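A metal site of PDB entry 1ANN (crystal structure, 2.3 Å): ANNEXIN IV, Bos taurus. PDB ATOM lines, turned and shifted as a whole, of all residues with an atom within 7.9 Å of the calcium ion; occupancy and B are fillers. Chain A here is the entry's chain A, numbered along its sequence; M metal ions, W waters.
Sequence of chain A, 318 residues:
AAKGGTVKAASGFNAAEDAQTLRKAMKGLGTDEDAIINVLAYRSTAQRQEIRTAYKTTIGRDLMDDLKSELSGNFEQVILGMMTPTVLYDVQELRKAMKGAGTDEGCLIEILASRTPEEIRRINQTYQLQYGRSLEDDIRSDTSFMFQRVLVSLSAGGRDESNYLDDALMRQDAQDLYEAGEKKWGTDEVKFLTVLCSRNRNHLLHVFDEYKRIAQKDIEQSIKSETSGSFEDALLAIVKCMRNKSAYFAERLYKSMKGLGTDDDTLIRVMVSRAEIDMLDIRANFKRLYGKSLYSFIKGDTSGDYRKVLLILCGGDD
OG1 of Thr 31 sits close to OE1 of Glu 70, at 2.6 Å.
The calcium ion is bound by O of Gly 30, O of Gly 28, O of Met 26, OE2 of Glu 70, water W2, OE1 of Glu 70 and water W1. The calcium ion has seven donor atoms within binding distance.
Of the 13 residues printed, 4 come within 4 Å of the calcium ion. The nearest printed residue that does not touch the calcium ion is Leu 29 (4.2 Å).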
ATOM      1  N   ARG A  23      -0.374  27.637   9.423  1.00  0.00           N
ATOM      2  CA  ARG A  23       0.568  28.746   9.220  1.00  0.00           C
ATOM      3  C   ARG A  23       1.995  28.357   9.620  1.00  0.00           C
ATOM      4  O   ARG A  23       2.950  28.570   8.880  1.00  0.00           O
ATOM      5  CB  ARG A  23       0.106  29.986  10.016  1.00  0.00           C
ATOM      6  CG  ARG A  23       1.083  31.148  10.038  1.00  0.00           C
ATOM      7  CD  ARG A  23       1.401  31.695   8.648  1.00  0.00           C
ATOM      8  NE  ARG A  23       2.211  32.907   8.762  1.00  0.00           N
ATOM      9  CZ  ARG A  23       2.953  33.442   7.781  1.00  0.00           C
ATOM     10  NH1 ARG A  23       3.018  32.884   6.579  1.00  0.00           N
ATOM     11  NH2 ARG A  23       3.664  34.522   8.030  1.00  0.00           N
ATOM     12  N   LYS A  24       2.132  27.739  10.775  1.00  0.00           N
ATOM     13  CA  LYS A  24       3.442  27.330  11.225  1.00  0.00           C
ATOM     14  C   LYS A  24       4.042  26.268  10.284  1.00  0.00           C
ATOM     15  O   LYS A  24       5.255  26.202  10.083  1.00  0.00           O
ATOM     16  CB  LYS A  24       3.334  26.796  12.660  1.00  0.00           C
ATOM     17  CG  LYS A  24       4.667  26.356  13.227  1.00  0.00           C
ATOM     18  CD  LYS A  24       4.523  25.787  14.620  1.00  0.00           C
ATOM     19  CE  LYS A  24       5.864  25.295  15.123  1.00  0.00           C
ATOM     20  NZ  LYS A  24       5.790  24.621  16.457  1.00  0.00           N
ATOM     21  N   ALA A  25       3.197  25.437   9.672  1.00  0.00           N
ATOM     22  CA  ALA A  25       3.671  24.398   8.765  1.00  0.00           C
ATOM     23  C   ALA A  25       4.172  24.976   7.445  1.00  0.00           C
ATOM     24  O   ALA A  25       5.018  24.390   6.774  1.00  0.00           O
ATOM     25  CB  ALA A  25       2.569  23.378   8.511  1.00  0.00           C
ATOM     26  N   MET A  26       3.618  26.127   7.043  1.00  0.00           N
ATOM     27  CA  MET A  26       3.992  26.765   5.781  1.00  0.00           C
ATOM     28  C   MET A  26       4.971  27.923   5.879  1.00  0.00           C
ATOM     29  O   MET A  26       5.628  28.285   4.901  1.00  0.00           O
ATOM     30  CB  MET A  26       2.734  27.221   5.032  1.00  0.00           C
ATOM     31  CG  MET A  26       1.857  26.079   4.596  1.00  0.00           C
ATOM     32  SD  MET A  26       0.453  26.653   3.673  1.00  0.00           S
ATOM     33  CE  MET A  26      -0.621  27.213   4.997  1.00  0.00           C
ATOM     34  N   LYS A  27       5.040  28.559   7.041  1.00  0.00           N
ATOM     35  CA  LYS A  27       5.931  29.690   7.222  1.00  0.00           C
ATOM     36  C   LYS A  27       7.379  29.283   7.004  1.00  0.00           C
ATOM     37  O   LYS A  27       7.801  28.208   7.437  1.00  0.00           O
ATOM     38  CB  LYS A  27       5.743  30.275   8.615  1.00  0.00           C
ATOM     39  CG  LYS A  27       6.229  31.692   8.788  1.00  0.00           C
ATOM     40  CD  LYS A  27       5.958  32.115  10.221  1.00  0.00           C
ATOM     41  CE  LYS A  27       6.347  33.557  10.495  1.00  0.00           C
ATOM     42  NZ  LYS A  27       5.991  33.845  11.909  1.00  0.00           N
ATOM     43  N   GLY A  28       8.118  30.149   6.326  1.00  0.00           N
ATOM     44  CA  GLY A  28       9.519  29.896   6.084  1.00  0.00           C
ATOM     45  C   GLY A  28       9.805  29.242   4.753  1.00  0.00           C
ATOM     46  O   GLY A  28       8.932  29.029   3.928  1.00  0.00           O
ATOM     47  N   LEU A  29      11.070  28.948   4.531  1.00  0.00           N
ATOM     48  CA  LEU A  29      11.493  28.318   3.310  1.00  0.00           C
ATOM     49  C   LEU A  29      11.082  26.852   3.429  1.00  0.00           C
ATOM     50  O   LEU A  29      11.456  26.177   4.394  1.00  0.00           O
ATOM     51  CB  LEU A  29      13.002  28.448   3.187  1.00  0.00           C
ATOM     52  CG  LEU A  29      13.581  28.649   1.787  1.00  0.00           C
ATOM     53  CD1 LEU A  29      13.223  30.023   1.242  1.00  0.00           C
ATOM     54  CD2 LEU A  29      15.083  28.497   1.894  1.00  0.00           C
ATOM     55  N   GLY A  30      10.297  26.355   2.482  1.00  0.00           N
ATOM     56  CA  GLY A  30       9.859  24.969   2.535  1.00  0.00           C
ATOM     57  C   GLY A  30       8.467  24.805   3.116  1.00  0.00           C
ATOM     58  O   GLY A  30       7.772  25.787   3.356  1.00  0.00           O
ATOM     59  N   THR A  31       8.086  23.566   3.392  1.00  0.00           N
ATOM     60  CA  THR A  31       6.745  23.261   3.899  1.00  0.00           C
ATOM     61  C   THR A  31       6.749  21.985   4.683  1.00  0.00           C
ATOM     62  O   THR A  31       7.456  21.035   4.336  1.00  0.00           O
ATOM     63  CB  THR A  31       5.803  23.011   2.732  1.00  0.00           C
ATOM     64  OG1 THR A  31       5.930  24.082   1.789  1.00  0.00           O
ATOM     65  CG2 THR A  31       4.338  22.876   3.182  1.00  0.00           C
ATOM     66  N   ASP A  32       5.947  21.959   5.742  1.00  0.00           N
ATOM     67  CA  ASP A  32       5.797  20.751   6.552  1.00  0.00           C
ATOM     68  C   ASP A  32       4.512  20.082   6.030  1.00  0.00           C
ATOM     69  O   ASP A  32       3.439  20.294   6.577  1.00  0.00           O
ATOM     70  CB  ASP A  32       5.644  21.092   8.025  1.00  0.00           C
ATOM     71  CG  ASP A  32       5.697  19.864   8.926  1.00  0.00           C
ATOM     72  OD1 ASP A  32       5.746  18.725   8.403  1.00  0.00           O
ATOM     73  OD2 ASP A  32       5.703  20.033  10.161  1.00  0.00           O
ATOM     74  N   ASP A  66      -2.053  30.309  -0.021  1.00  0.00           N
ATOM     75  CA  ASP A  66      -0.876  29.718   0.606  1.00  0.00           C
ATOM     76  C   ASP A  66      -0.751  28.245   0.242  1.00  0.00           C
ATOM     77  O   ASP A  66       0.352  27.760  -0.020  1.00  0.00           O
ATOM     78  CB  ASP A  66      -0.955  29.851   2.121  1.00  0.00           C
ATOM     79  CG  ASP A  66      -0.514  31.202   2.604  1.00  0.00           C
ATOM     80  OD1 ASP A  66       0.148  31.930   1.836  1.00  0.00           O
ATOM     81  OD2 ASP A  66      -0.823  31.528   3.765  1.00  0.00           O
ATOM     82  N   SER A  69       0.484  28.214  -3.411  1.00  0.00           N
ATOM     83  CA  SER A  69       1.876  28.594  -3.580  1.00  0.00           C
ATOM     84  C   SER A  69       2.831  27.620  -2.903  1.00  0.00           C
ATOM     85  O   SER A  69       3.908  27.344  -3.437  1.00  0.00           O
ATOM     86  CB  SER A  69       2.124  30.028  -3.107  1.00  0.00           C
ATOM     87  OG  SER A  69       2.304  30.111  -1.710  1.00  0.00           O
ATOM     88  N   GLU A  70       2.415  27.064  -1.778  1.00  0.00           N
ATOM     89  CA  GLU A  70       3.245  26.112  -1.022  1.00  0.00           C
ATOM     90  C   GLU A  70       3.315  24.694  -1.560  1.00  0.00           C
ATOM     91  O   GLU A  70       4.326  24.025  -1.371  1.00  0.00           O
ATOM     92  CB  GLU A  70       2.778  26.038   0.427  1.00  0.00           C
ATOM     93  CG  GLU A  70       2.995  27.300   1.240  1.00  0.00           C
ATOM     94  CD  GLU A  70       4.439  27.453   1.698  1.00  0.00           C
ATOM     95  OE1 GLU A  70       5.009  26.469   2.211  1.00  0.00           O
ATOM     96  OE2 GLU A  70       4.989  28.559   1.604  1.00  0.00           O
HETATM   97 CA    CA M   1       7.048  27.971   3.012  1.00  0.00          CA
HETATM   98  O   HOH W   1       8.013  27.599   0.513  1.00  0.00           O
HETATM   99  O   HOH W   2       7.378  30.481   2.281  1.00  0.00           O
